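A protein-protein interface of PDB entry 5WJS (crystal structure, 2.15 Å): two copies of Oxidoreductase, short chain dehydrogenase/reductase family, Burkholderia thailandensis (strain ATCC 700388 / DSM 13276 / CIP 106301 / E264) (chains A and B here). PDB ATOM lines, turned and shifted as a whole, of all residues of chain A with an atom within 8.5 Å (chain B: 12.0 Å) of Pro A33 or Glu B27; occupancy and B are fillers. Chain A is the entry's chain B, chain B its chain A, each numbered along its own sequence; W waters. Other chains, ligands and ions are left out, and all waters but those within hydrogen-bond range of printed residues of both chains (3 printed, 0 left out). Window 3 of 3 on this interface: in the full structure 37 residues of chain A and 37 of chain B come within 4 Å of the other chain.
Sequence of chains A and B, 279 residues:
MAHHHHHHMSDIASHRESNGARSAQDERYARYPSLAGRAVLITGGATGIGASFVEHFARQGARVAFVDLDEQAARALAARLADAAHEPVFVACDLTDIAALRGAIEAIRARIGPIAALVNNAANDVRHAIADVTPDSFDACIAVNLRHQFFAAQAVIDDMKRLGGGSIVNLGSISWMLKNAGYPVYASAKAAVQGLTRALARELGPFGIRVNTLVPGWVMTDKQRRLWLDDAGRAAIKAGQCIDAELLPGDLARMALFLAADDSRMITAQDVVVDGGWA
OD2 of Asp A262 lies within salt-bridge range of NE of Arg B28 (3.3 Å).
OD2 of Asp A263 sits at hydrogen-bond distance from N of Ala B30, at 2.8 Å.
O of Arg B31 lies within hydrogen-bond range of N of Arg A31 (3.4 Å).
The guanidinium group of Arg B254 is in hydrogen-bond range of the backbone carbonyl oxygen of Asp A263 (3.0 Å).
The side-chain carboxylate of Asp B263 lies within hydrogen-bond range of the backbone NH of Ala A30.
The backbone carbonyl oxygen (O) of Ala B30 lies within hydrogen-bond range of the side-chain amide nitrogen (NE2) of Gln B60 (3.1 Å).
N of Tyr B32 sits at hydrogen-bond distance from OE1 of Gln B60, at 2.8 Å.
NE2 of Gln A60 lies within hydrogen-bond range of O of Ala A30 (3.2 Å).
The side-chain amide oxygen (OE1) of Gln A60 is in hydrogen-bond range of the backbone NH (N) of Tyr A32.
N of Asp A262 is in hydrogen-bond range of OG of Ser A34.
NH2 of Arg A38 is in salt-bridge range of OD1 of Asp A262, at 2.9 Å.
CB of Ala A30 touches CD2 of Tyr B32 (3.7 Å).
CA of Ala A30 touches CD of Pro B33 (3.96 Å).
Arg A31 touches Ala B30.
Tyr A32 touches Phe B258.
Pro A33 touches Glu B27.
Pro A33 touches Arg B28 (CD to O, 3.4 Å).
Pro A33 touches Tyr B29 (CD to O, 3.2 Å).
Pro A33 touches Ala B30 (CD to CA, 3.995 Å).
Tyr B29 touches Asp A262.
OD2 of Asp A263 touches CA of Tyr B29, 3.6 Å away.
Of the printed residues of chain B, Pro A33 touches Glu B27, Arg B28, Tyr B29 and Ala B30.
Glu B27 touches just one residue of chain A: Pro A33.
Arg A31 touches just these residues of chain B: Ala B30 (3.3 Å) and Arg B31 (3.4 Å).
No residue of chain B comes within 4 Å of Gly A61.
Of the printed residues of chain A, Phe B258 touches Tyr A32 (3.4 Å).
Printed residues of chain A within 4 Å of Asp B263: Ala A30 (2.7 Å).
Of the printed residues of chain A, Tyr B29 touches Pro A33, Asp A262 and Asp A263.
Of the printed residues of chain A, Arg B28 touches Pro A33, Ser A34 and Asp A262.
Ser B23 touches none of the printed residues of chain A.
The nearest residue of chain A that does not touch Glu B27 is Ser A34 (5.8 Å).
The nearest printed residue of chain B that does not touch Tyr A32 is Tyr B32 (4.4 Å).
Printed residues of chain B that touch a printed residue of chain A: Glu B27, Arg B28, Tyr B29, Ala B30, Arg B31, Tyr B32, Pro B33, Arg B254, Phe B258 and Asp B263.
Hydrophobic or aromatic side chains of chain B that line the printed part of chain A: Tyr B29, Ala B30, Tyr B32, Pro B33 and Phe B258.
Along chain B the printed residues that touch a printed residue of chain A span positions 27 to 263.
Of the 15 printed residues of chain A, 7 touch a printed residue of chain B.
Printed residues of chain A that touch a printed residue of chain B: Ala A30, Arg A31, Tyr A32, Pro A33, Ser A34, Asp A262 and Asp A263.
Among the printed residues, Asp or Glu carboxylates within 4 Å of a Lys or Arg side-chain nitrogen of the other chain: Asp A262 with Arg B28.
Ala A30 touches Arg B31, and with the chains exchanged Arg A31 touches Ala B30.
Ala A30 touches Tyr B32, and with the chains exchanged Tyr A32 touches Ala B30.
Ala A30 touches Pro B33, and with the chains exchanged Pro A33 touches Ala B30.
Ala A30 touches Asp B263, and with the chains exchanged Asp A263 touches Ala B30.
Positions printed for both chains: 30, 31, 32, 33, 60 and 263.
Of the 18 pairs that touch across the chains among the printed residues, 9 have their exchanged pair printed and touching as well.
Water W2 bridges OH of Tyr A32 and OD2 of Asp B263.
Water W3 lies within hydrogen-bond range of OG of Ser A34 (2.6 Å), OD1 of Asp A263 (2.7 Å) and O of Arg B28 (2.7 Å).
Water W1 bridges the side-chain hydroxyl (OH) of Tyr B32 (2.7 Å) and the side-chain carboxylate (OD2) of Asp A263 (2.8 Å).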
ATOM      1  N   ALA A  30     -10.583  35.717 -10.384  1.00  0.00           N
ATOM      2  CA  ALA A  30     -10.023  34.822 -11.389  1.00  0.00           C
ATOM      3  C   ALA A  30      -9.712  35.542 -12.699  1.00  0.00           C
ATOM      4  O   ALA A  30     -10.303  36.572 -13.040  1.00  0.00           O
ATOM      5  CB  ALA A  30     -10.984  33.674 -11.673  1.00  0.00           C
ATOM      6  N   ARG A  31      -8.768  34.974 -13.445  1.00  0.00           N
ATOM      7  CA  ARG A  31      -8.539  35.341 -14.831  1.00  0.00           C
ATOM      8  C   ARG A  31      -8.795  34.104 -15.678  1.00  0.00           C
ATOM      9  O   ARG A  31      -8.397  32.996 -15.303  1.00  0.00           O
ATOM     10  CB  ARG A  31      -7.111  35.885 -15.043  1.00  0.00           C
ATOM     11  N   TYR A  32      -9.496  34.289 -16.799  1.00  0.00           N
ATOM     12  CA  TYR A  32      -9.962  33.178 -17.624  1.00  0.00           C
ATOM     13  C   TYR A  32      -9.238  33.211 -18.959  1.00  0.00           C
ATOM     14  O   TYR A  32      -9.619  33.984 -19.853  1.00  0.00           O
ATOM     15  CB  TYR A  32     -11.476  33.262 -17.838  1.00  0.00           C
ATOM     16  CG  TYR A  32     -12.284  33.190 -16.568  1.00  0.00           C
ATOM     17  CD1 TYR A  32     -12.571  34.342 -15.830  1.00  0.00           C
ATOM     18  CD2 TYR A  32     -12.764  31.971 -16.101  1.00  0.00           C
ATOM     19  CE1 TYR A  32     -13.317  34.274 -14.655  1.00  0.00           C
ATOM     20  CE2 TYR A  32     -13.506  31.895 -14.937  1.00  0.00           C
ATOM     21  CZ  TYR A  32     -13.778  33.047 -14.217  1.00  0.00           C
ATOM     22  OH  TYR A  32     -14.517  32.952 -13.054  1.00  0.00           O
ATOM     23  N   PRO A  33      -8.201  32.394 -19.153  1.00  0.00           N
ATOM     24  CA  PRO A  33      -7.374  32.546 -20.364  1.00  0.00           C
ATOM     25  C   PRO A  33      -8.167  32.360 -21.637  1.00  0.00           C
ATOM     26  O   PRO A  33      -7.897  33.047 -22.632  1.00  0.00           O
ATOM     27  CB  PRO A  33      -6.294  31.463 -20.196  1.00  0.00           C
ATOM     28  CG  PRO A  33      -6.270  31.155 -18.710  1.00  0.00           C
ATOM     29  CD  PRO A  33      -7.725  31.307 -18.279  1.00  0.00           C
ATOM     30  N   SER A  34      -9.182  31.492 -21.613  1.00  0.00           N
ATOM     31  CA  SER A  34     -10.005  31.215 -22.786  1.00  0.00           C
ATOM     32  C   SER A  34     -10.871  32.397 -23.208  1.00  0.00           C
ATOM     33  O   SER A  34     -11.409  32.377 -24.319  1.00  0.00           O
ATOM     34  CB  SER A  34     -10.893  29.992 -22.522  1.00  0.00           C
ATOM     35  OG  SER A  34     -11.840  30.250 -21.505  1.00  0.00           O
ATOM     36  N   LEU A  35     -11.024  33.423 -22.373  1.00  0.00           N
ATOM     37  CA  LEU A  35     -11.779  34.585 -22.826  1.00  0.00           C
ATOM     38  C   LEU A  35     -10.944  35.549 -23.664  1.00  0.00           C
ATOM     39  O   LEU A  35     -11.521  36.390 -24.362  1.00  0.00           O
ATOM     40  CB  LEU A  35     -12.383  35.343 -21.634  1.00  0.00           C
ATOM     41  CG  LEU A  35     -13.363  34.562 -20.763  1.00  0.00           C
ATOM     42  CD1 LEU A  35     -13.971  35.445 -19.650  1.00  0.00           C
ATOM     43  CD2 LEU A  35     -14.456  33.929 -21.626  1.00  0.00           C
ATOM     44  N   ALA A  36      -9.614  35.459 -23.614  1.00  0.00           N
ATOM     45  CA  ALA A  36      -8.763  36.429 -24.300  1.00  0.00           C
ATOM     46  C   ALA A  36      -8.980  36.344 -25.803  1.00  0.00           C
ATOM     47  O   ALA A  36      -8.827  35.275 -26.399  1.00  0.00           O
ATOM     48  CB  ALA A  36      -7.291  36.185 -23.962  1.00  0.00           C
ATOM     49  N   GLY A  37      -9.327  37.470 -26.416  1.00  0.00           N
ATOM     50  CA  GLY A  37      -9.661  37.499 -27.826  1.00  0.00           C
ATOM     51  C   GLY A  37     -11.014  36.916 -28.190  1.00  0.00           C
ATOM     52  O   GLY A  37     -11.397  36.977 -29.365  1.00  0.00           O
ATOM     53  N   ARG A  38     -11.760  36.369 -27.231  1.00  0.00           N
ATOM     54  CA  ARG A  38     -13.030  35.729 -27.555  1.00  0.00           C
ATOM     55  C   ARG A  38     -14.097  36.772 -27.898  1.00  0.00           C
ATOM     56  O   ARG A  38     -14.249  37.780 -27.202  1.00  0.00           O
ATOM     57  CB  ARG A  38     -13.485  34.841 -26.391  1.00  0.00           C
ATOM     58  CG  ARG A  38     -14.929  34.299 -26.546  1.00  0.00           C
ATOM     59  CD  ARG A  38     -15.156  33.002 -25.753  1.00  0.00           C
ATOM     60  NE  ARG A  38     -14.208  31.953 -26.134  1.00  0.00           N
ATOM     61  CZ  ARG A  38     -14.024  30.827 -25.452  1.00  0.00           C
ATOM     62  NH1 ARG A  38     -14.723  30.597 -24.342  1.00  0.00           N
ATOM     63  NH2 ARG A  38     -13.129  29.933 -25.867  1.00  0.00           N
ATOM     64  N   GLN A  60     -11.028  41.002 -19.157  1.00  0.00           N
ATOM     65  CA  GLN A  60     -10.494  39.657 -19.338  1.00  0.00           C
ATOM     66  C   GLN A  60      -9.786  39.480 -20.681  1.00  0.00           C
ATOM     67  O   GLN A  60      -9.216  38.409 -20.938  1.00  0.00           O
ATOM     68  CB  GLN A  60     -11.612  38.622 -19.193  1.00  0.00           C
ATOM     69  CG  GLN A  60     -12.210  38.546 -17.778  1.00  0.00           C
ATOM     70  CD  GLN A  60     -11.261  37.901 -16.770  1.00  0.00           C
ATOM     71  OE1 GLN A  60     -10.435  37.042 -17.123  1.00  0.00           O
ATOM     72  NE2 GLN A  60     -11.368  38.318 -15.509  1.00  0.00           N
ATOM     73  N   GLY A  61      -9.785  40.500 -21.529  1.00  0.00           N
ATOM     74  CA  GLY A  61      -9.169  40.396 -22.832  1.00  0.00           C
ATOM     75  C   GLY A  61     -10.106  39.999 -23.943  1.00  0.00           C
ATOM     76  O   GLY A  61      -9.639  39.729 -25.051  1.00  0.00           O
ATOM     77  N   ALA A  62     -11.415  39.945 -23.685  1.00  0.00           N
ATOM     78  CA  ALA A  62     -12.329  39.541 -24.740  1.00  0.00           C
ATOM     79  C   ALA A  62     -12.515  40.673 -25.744  1.00  0.00           C
ATOM     80  O   ALA A  62     -12.205  41.840 -25.485  1.00  0.00           O
ATOM     81  CB  ALA A  62     -13.683  39.112 -24.166  1.00  0.00           C
ATOM     82  N   ALA A 261     -16.672  31.098 -20.291  1.00  0.00           N
ATOM     83  CA  ALA A 261     -15.331  30.555 -20.469  1.00  0.00           C
ATOM     84  C   ALA A 261     -15.390  29.045 -20.690  1.00  0.00           C
ATOM     85  O   ALA A 261     -16.404  28.388 -20.421  1.00  0.00           O
ATOM     86  CB  ALA A 261     -14.451  30.870 -19.251  1.00  0.00           C
ATOM     87  N   ASP A 262     -14.266  28.483 -21.162  1.00  0.00           N
ATOM     88  CA  ASP A 262     -14.191  27.038 -21.346  1.00  0.00           C
ATOM     89  C   ASP A 262     -14.413  26.275 -20.043  1.00  0.00           C
ATOM     90  O   ASP A 262     -14.739  25.083 -20.089  1.00  0.00           O
ATOM     91  CB  ASP A 262     -12.836  26.617 -21.905  1.00  0.00           C
ATOM     92  CG  ASP A 262     -12.571  27.127 -23.322  1.00  0.00           C
ATOM     93  OD1 ASP A 262     -13.429  27.781 -23.938  1.00  0.00           O
ATOM     94  OD2 ASP A 262     -11.456  26.882 -23.804  1.00  0.00           O
ATOM     95  N   ASP A 263     -14.231  26.930 -18.891  1.00  0.00           N
ATOM     96  CA  ASP A 263     -14.307  26.261 -17.592  1.00  0.00           C
ATOM     97  C   ASP A 263     -15.653  25.590 -17.336  1.00  0.00           C
ATOM     98  O   ASP A 263     -15.727  24.673 -16.508  1.00  0.00           O
ATOM     99  CB  ASP A 263     -14.014  27.278 -16.482  1.00  0.00           C
ATOM    100  CG  ASP A 263     -12.679  27.981 -16.688  1.00  0.00           C
ATOM    101  OD1 ASP A 263     -12.541  28.705 -17.691  1.00  0.00           O
ATOM    102  OD2 ASP A 263     -11.763  27.783 -15.865  1.00  0.00           O
ATOM    103  N   ARG B  22      -2.943  16.695 -17.919  1.00  0.00           N
ATOM    104  CA  ARG B  22      -3.825  16.769 -16.756  1.00  0.00           C
ATOM    105  C   ARG B  22      -4.783  17.950 -16.863  1.00  0.00           C
ATOM    106  O   ARG B  22      -4.366  19.075 -17.144  1.00  0.00           O
ATOM    107  CB  ARG B  22      -3.023  16.892 -15.458  1.00  0.00           C
ATOM    108  CG  ARG B  22      -2.101  15.730 -15.161  1.00  0.00           C
ATOM    109  CD  ARG B  22      -2.866  14.426 -15.026  1.00  0.00           C
ATOM    110  NE  ARG B  22      -3.888  14.470 -13.985  1.00  0.00           N
ATOM    111  CZ  ARG B  22      -4.562  13.403 -13.570  1.00  0.00           C
ATOM    112  NH1 ARG B  22      -4.310  12.217 -14.107  1.00  0.00           N
ATOM    113  NH2 ARG B  22      -5.481  13.512 -12.620  1.00  0.00           N
ATOM    114  N   SER B  23      -6.069  17.689 -16.617  1.00  0.00           N
ATOM    115  CA  SER B  23      -7.057  18.761 -16.671  1.00  0.00           C
ATOM    116  C   SER B  23      -6.774  19.842 -15.631  1.00  0.00           C
ATOM    117  O   SER B  23      -6.997  21.028 -15.900  1.00  0.00           O
ATOM    118  CB  SER B  23      -8.463  18.183 -16.481  1.00  0.00           C
ATOM    119  OG  SER B  23      -9.462  19.168 -16.684  1.00  0.00           O
ATOM    120  N   ALA B  24      -6.266  19.461 -14.450  1.00  0.00           N
ATOM    121  CA  ALA B  24      -6.050  20.429 -13.376  1.00  0.00           C
ATOM    122  C   ALA B  24      -4.922  21.410 -13.676  1.00  0.00           C
ATOM    123  O   ALA B  24      -4.856  22.468 -13.040  1.00  0.00           O
ATOM    124  CB  ALA B  24      -5.760  19.708 -12.061  1.00  0.00           C
ATOM    125  N   GLN B  25      -4.037  21.095 -14.621  1.00  0.00           N
ATOM    126  CA  GLN B  25      -2.974  22.009 -15.015  1.00  0.00           C
ATOM    127  C   GLN B  25      -3.163  22.551 -16.426  1.00  0.00           C
ATOM    128  O   GLN B  25      -2.242  23.170 -16.971  1.00  0.00           O
ATOM    129  CB  GLN B  25      -1.612  21.323 -14.893  1.00  0.00           C
ATOM    130  CG  GLN B  25      -1.249  20.908 -13.483  1.00  0.00           C
ATOM    131  CD  GLN B  25      -0.014  20.021 -13.440  1.00  0.00           C
ATOM    132  OE1 GLN B  25      -0.078  18.831 -13.762  1.00  0.00           O
ATOM    133  NE2 GLN B  25       1.118  20.600 -13.052  1.00  0.00           N
ATOM    134  N   ASP B  26      -4.327  22.329 -17.035  1.00  0.00           N
ATOM    135  CA  ASP B  26      -4.561  22.814 -18.391  1.00  0.00           C
ATOM    136  C   ASP B  26      -4.546  24.341 -18.402  1.00  0.00           C
ATOM    137  O   ASP B  26      -5.317  24.989 -17.684  1.00  0.00           O
ATOM    138  CB  ASP B  26      -5.895  22.280 -18.921  1.00  0.00           C
ATOM    139  CG  ASP B  26      -6.056  22.486 -20.418  1.00  0.00           C
ATOM    140  OD1 ASP B  26      -6.418  21.516 -21.117  1.00  0.00           O
ATOM    141  OD2 ASP B  26      -5.812  23.610 -20.905  1.00  0.00           O
ATOM    142  N   GLU B  27      -3.671  24.910 -19.231  1.00  0.00           N
ATOM    143  CA  GLU B  27      -3.456  26.352 -19.244  1.00  0.00           C
ATOM    144  C   GLU B  27      -4.674  27.132 -19.736  1.00  0.00           C
ATOM    145  O   GLU B  27      -4.745  28.345 -19.514  1.00  0.00           O
ATOM    146  CB  GLU B  27      -2.239  26.688 -20.111  1.00  0.00           C
ATOM    147  N   ARG B  28      -5.631  26.481 -20.400  1.00  0.00           N
ATOM    148  CA  ARG B  28      -6.809  27.204 -20.859  1.00  0.00           C
ATOM    149  C   ARG B  28      -7.770  27.562 -19.722  1.00  0.00           C
ATOM    150  O   ARG B  28      -8.618  28.439 -19.906  1.00  0.00           O
ATOM    151  CB  ARG B  28      -7.544  26.385 -21.920  1.00  0.00           C
ATOM    152  CG  ARG B  28      -8.787  25.704 -21.394  1.00  0.00           C
ATOM    153  CD  ARG B  28      -8.954  24.310 -21.962  1.00  0.00           C
ATOM    154  NE  ARG B  28      -9.425  24.311 -23.337  1.00  0.00           N
ATOM    155  CZ  ARG B  28      -9.433  23.231 -24.109  1.00  0.00           C
ATOM    156  NH1 ARG B  28      -9.873  23.306 -25.359  1.00  0.00           N
ATOM    157  NH2 ARG B  28      -8.990  22.073 -23.628  1.00  0.00           N
ATOM    158  N   TYR B  29      -7.654  26.930 -18.557  1.00  0.00           N
ATOM    159  CA  TYR B  29      -8.637  27.111 -17.492  1.00  0.00           C
ATOM    160  C   TYR B  29      -8.203  28.215 -16.525  1.00  0.00           C
ATOM    161  O   TYR B  29      -7.069  28.695 -16.552  1.00  0.00           O
ATOM    162  CB  TYR B  29      -8.874  25.792 -16.741  1.00  0.00           C
ATOM    163  CG  TYR B  29      -9.549  24.754 -17.602  1.00  0.00           C
ATOM    164  CD1 TYR B  29     -10.709  25.063 -18.298  1.00  0.00           C
ATOM    165  CD2 TYR B  29      -9.014  23.476 -17.747  1.00  0.00           C
ATOM    166  CE1 TYR B  29     -11.323  24.133 -19.105  1.00  0.00           C
ATOM    167  CE2 TYR B  29      -9.623  22.533 -18.560  1.00  0.00           C
ATOM    168  CZ  TYR B  29     -10.785  22.872 -19.233  1.00  0.00           C
ATOM    169  OH  TYR B  29     -11.417  21.961 -20.048  1.00  0.00           O
ATOM    170  N   ALA B  30      -9.135  28.618 -15.667  1.00  0.00           N
ATOM    171  CA  ALA B  30      -8.942  29.772 -14.797  1.00  0.00           C
ATOM    172  C   ALA B  30      -7.979  29.485 -13.648  1.00  0.00           C
ATOM    173  O   ALA B  30      -7.930  28.382 -13.097  1.00  0.00           O
ATOM    174  CB  ALA B  30     -10.279  30.227 -14.211  1.00  0.00           C
ATOM    175  N   ARG B  31      -7.247  30.522 -13.255  1.00  0.00           N
ATOM    176  CA  ARG B  31      -6.466  30.534 -12.023  1.00  0.00           C
ATOM    177  C   ARG B  31      -7.159  31.466 -11.035  1.00  0.00           C
ATOM    178  O   ARG B  31      -7.532  32.589 -11.396  1.00  0.00           O
ATOM    179  CB  ARG B  31      -5.018  30.985 -12.286  1.00  0.00           C
ATOM    180  N   TYR B  32      -7.354  30.993  -9.799  1.00  0.00           N
ATOM    181  CA  TYR B  32      -8.091  31.736  -8.774  1.00  0.00           C
ATOM    182  C   TYR B  32      -7.116  32.254  -7.730  1.00  0.00           C
ATOM    183  O   TYR B  32      -6.713  31.494  -6.837  1.00  0.00           O
ATOM    184  CB  TYR B  32      -9.147  30.844  -8.111  1.00  0.00           C
ATOM    185  CG  TYR B  32     -10.199  30.317  -9.060  1.00  0.00           C
ATOM    186  CD1 TYR B  32      -9.970  29.175  -9.821  1.00  0.00           C
ATOM    187  CD2 TYR B  32     -11.418  30.973  -9.208  1.00  0.00           C
ATOM    188  CE1 TYR B  32     -10.934  28.691 -10.694  1.00  0.00           C
ATOM    189  CE2 TYR B  32     -12.380  30.506 -10.081  1.00  0.00           C
ATOM    190  CZ  TYR B  32     -12.136  29.361 -10.820  1.00  0.00           C
ATOM    191  OH  TYR B  32     -13.093  28.891 -11.687  1.00  0.00           O
ATOM    192  N   PRO B  33      -6.702  33.528  -7.789  1.00  0.00           N
ATOM    193  CA  PRO B  33      -5.637  33.983  -6.877  1.00  0.00           C
ATOM    194  C   PRO B  33      -5.994  33.821  -5.417  1.00  0.00           C
ATOM    195  O   PRO B  33      -5.103  33.596  -4.590  1.00  0.00           O
ATOM    196  CB  PRO B  33      -5.460  35.463  -7.251  1.00  0.00           C
ATOM    197  CG  PRO B  33      -5.936  35.560  -8.663  1.00  0.00           C
ATOM    198  CD  PRO B  33      -7.088  34.578  -8.749  1.00  0.00           C
ATOM    199  N   GLU B  55      -6.644  17.374  -6.432  1.00  0.00           N
ATOM    200  CA  GLU B  55      -5.678  17.729  -7.460  1.00  0.00           C
ATOM    201  C   GLU B  55      -5.868  19.167  -7.922  1.00  0.00           C
ATOM    202  O   GLU B  55      -4.894  19.916  -8.068  1.00  0.00           O
ATOM    203  CB  GLU B  55      -5.810  16.764  -8.633  1.00  0.00           C
ATOM    204  CG  GLU B  55      -4.836  17.052  -9.744  1.00  0.00           C
ATOM    205  CD  GLU B  55      -4.899  16.020 -10.847  1.00  0.00           C
ATOM    206  OE1 GLU B  55      -5.593  14.990 -10.672  1.00  0.00           O
ATOM    207  OE2 GLU B  55      -4.251  16.245 -11.887  1.00  0.00           O
ATOM    208  N   HIS B  56      -7.121  19.572  -8.155  1.00  0.00           N
ATOM    209  CA  HIS B  56      -7.382  20.929  -8.627  1.00  0.00           C
ATOM    210  C   HIS B  56      -6.991  21.956  -7.575  1.00  0.00           C
ATOM    211  O   HIS B  56      -6.235  22.889  -7.862  1.00  0.00           O
ATOM    212  CB  HIS B  56      -8.855  21.084  -9.045  1.00  0.00           C
ATOM    213  CG  HIS B  56      -9.135  20.559 -10.423  1.00  0.00           C
ATOM    214  ND1 HIS B  56      -9.235  19.211 -10.699  1.00  0.00           N
ATOM    215  CD2 HIS B  56      -9.287  21.197 -11.609  1.00  0.00           C
ATOM    216  CE1 HIS B  56      -9.473  19.044 -11.988  1.00  0.00           C
ATOM    217  NE2 HIS B  56      -9.506  20.232 -12.563  1.00  0.00           N
ATOM    218  N   ARG B  59      -3.320  22.246  -7.383  1.00  0.00           N
ATOM    219  CA  ARG B  59      -2.681  22.927  -8.504  1.00  0.00           C
ATOM    220  C   ARG B  59      -2.987  24.418  -8.525  1.00  0.00           C
ATOM    221  O   ARG B  59      -2.247  25.171  -9.160  1.00  0.00           O
ATOM    222  CB  ARG B  59      -3.090  22.285  -9.836  1.00  0.00           C
ATOM    223  CG  ARG B  59      -2.568  20.871 -10.039  1.00  0.00           C
ATOM    224  CD  ARG B  59      -1.037  20.828  -9.935  1.00  0.00           C
ATOM    225  NE  ARG B  59      -0.513  19.472 -10.090  1.00  0.00           N
ATOM    226  CZ  ARG B  59       0.689  19.080  -9.682  1.00  0.00           C
ATOM    227  NH1 ARG B  59       1.504  19.943  -9.079  1.00  0.00           N
ATOM    228  NH2 ARG B  59       1.079  17.827  -9.872  1.00  0.00           N
ATOM    229  N   GLN B  60      -4.054  24.861  -7.849  1.00  0.00           N
ATOM    230  CA  GLN B  60      -4.319  26.285  -7.661  1.00  0.00           C
ATOM    231  C   GLN B  60      -3.486  26.895  -6.540  1.00  0.00           C
ATOM    232  O   GLN B  60      -3.617  28.097  -6.278  1.00  0.00           O
ATOM    233  CB  GLN B  60      -5.802  26.526  -7.353  1.00  0.00           C
ATOM    234  CG  GLN B  60      -6.762  26.133  -8.470  1.00  0.00           C
ATOM    235  CD  GLN B  60      -6.711  27.082  -9.652  1.00  0.00           C
ATOM    236  OE1 GLN B  60      -6.541  28.290  -9.495  1.00  0.00           O
ATOM    237  NE2 GLN B  60      -6.850  26.534 -10.845  1.00  0.00           N
ATOM    238  N   ARG B 254     -13.645  22.178 -11.293  1.00  0.00           N
ATOM    239  CA  ARG B 254     -13.563  23.600 -11.614  1.00  0.00           C
ATOM    240  C   ARG B 254     -14.714  24.378 -10.990  1.00  0.00           C
ATOM    241  O   ARG B 254     -14.519  25.507 -10.531  1.00  0.00           O
ATOM    242  CB  ARG B 254     -13.513  23.805 -13.130  1.00  0.00           C
ATOM    243  CG  ARG B 254     -12.170  23.326 -13.749  1.00  0.00           C
ATOM    244  CD  ARG B 254     -12.033  23.722 -15.204  1.00  0.00           C
ATOM    245  NE  ARG B 254     -13.169  23.280 -16.015  1.00  0.00           N
ATOM    246  CZ  ARG B 254     -13.248  22.099 -16.627  1.00  0.00           C
ATOM    247  NH1 ARG B 254     -12.252  21.222 -16.525  1.00  0.00           N
ATOM    248  NH2 ARG B 254     -14.331  21.794 -17.345  1.00  0.00           N
ATOM    249  N   LEU B 257     -13.830  24.886  -7.378  1.00  0.00           N
ATOM    250  CA  LEU B 257     -12.834  25.950  -7.247  1.00  0.00           C
ATOM    251  C   LEU B 257     -13.505  27.315  -7.183  1.00  0.00           C
ATOM    252  O   LEU B 257     -13.221  28.123  -6.293  1.00  0.00           O
ATOM    253  CB  LEU B 257     -11.849  25.902  -8.421  1.00  0.00           C
ATOM    254  CG  LEU B 257     -10.832  24.765  -8.547  1.00  0.00           C
ATOM    255  CD1 LEU B 257      -9.957  25.033  -9.748  1.00  0.00           C
ATOM    256  CD2 LEU B 257      -9.963  24.582  -7.290  1.00  0.00           C
ATOM    257  N   PHE B 258     -14.407  27.579  -8.128  1.00  0.00           N
ATOM    258  CA  PHE B 258     -15.136  28.843  -8.160  1.00  0.00           C
ATOM    259  C   PHE B 258     -15.956  29.044  -6.891  1.00  0.00           C
ATOM    260  O   PHE B 258     -15.955  30.138  -6.308  1.00  0.00           O
ATOM    261  CB  PHE B 258     -16.018  28.867  -9.416  1.00  0.00           C
ATOM    262  CG  PHE B 258     -16.751  30.178  -9.654  1.00  0.00           C
ATOM    263  CD1 PHE B 258     -17.991  30.412  -9.060  1.00  0.00           C
ATOM    264  CD2 PHE B 258     -16.228  31.136 -10.508  1.00  0.00           C
ATOM    265  CE1 PHE B 258     -18.676  31.606  -9.296  1.00  0.00           C
ATOM    266  CE2 PHE B 258     -16.897  32.334 -10.753  1.00  0.00           C
ATOM    267  CZ  PHE B 258     -18.128  32.565 -10.142  1.00  0.00           C
ATOM    268  N   ASP B 263     -14.447  34.617  -5.716  1.00  0.00           N
ATOM    269  CA  ASP B 263     -15.292  35.007  -6.845  1.00  0.00           C
ATOM    270  C   ASP B 263     -16.775  34.709  -6.616  1.00  0.00           C
ATOM    271  O   ASP B 263     -17.627  35.301  -7.288  1.00  0.00           O
ATOM    272  CB  ASP B 263     -14.818  34.291  -8.115  1.00  0.00           C
ATOM    273  CG  ASP B 263     -13.323  34.454  -8.358  1.00  0.00           C
ATOM    274  OD1 ASP B 263     -12.518  34.083  -7.467  1.00  0.00           O
ATOM    275  OD2 ASP B 263     -12.960  34.954  -9.443  1.00  0.00           O
HETATM  276  O   HOH W   1     -12.156  26.868 -13.218  1.00  0.00           O
HETATM  277  O   HOH W   2     -14.538  35.162 -11.626  1.00  0.00           O
HETATM  278  O   HOH W   3     -10.685  30.000 -19.143  1.00  0.00           O
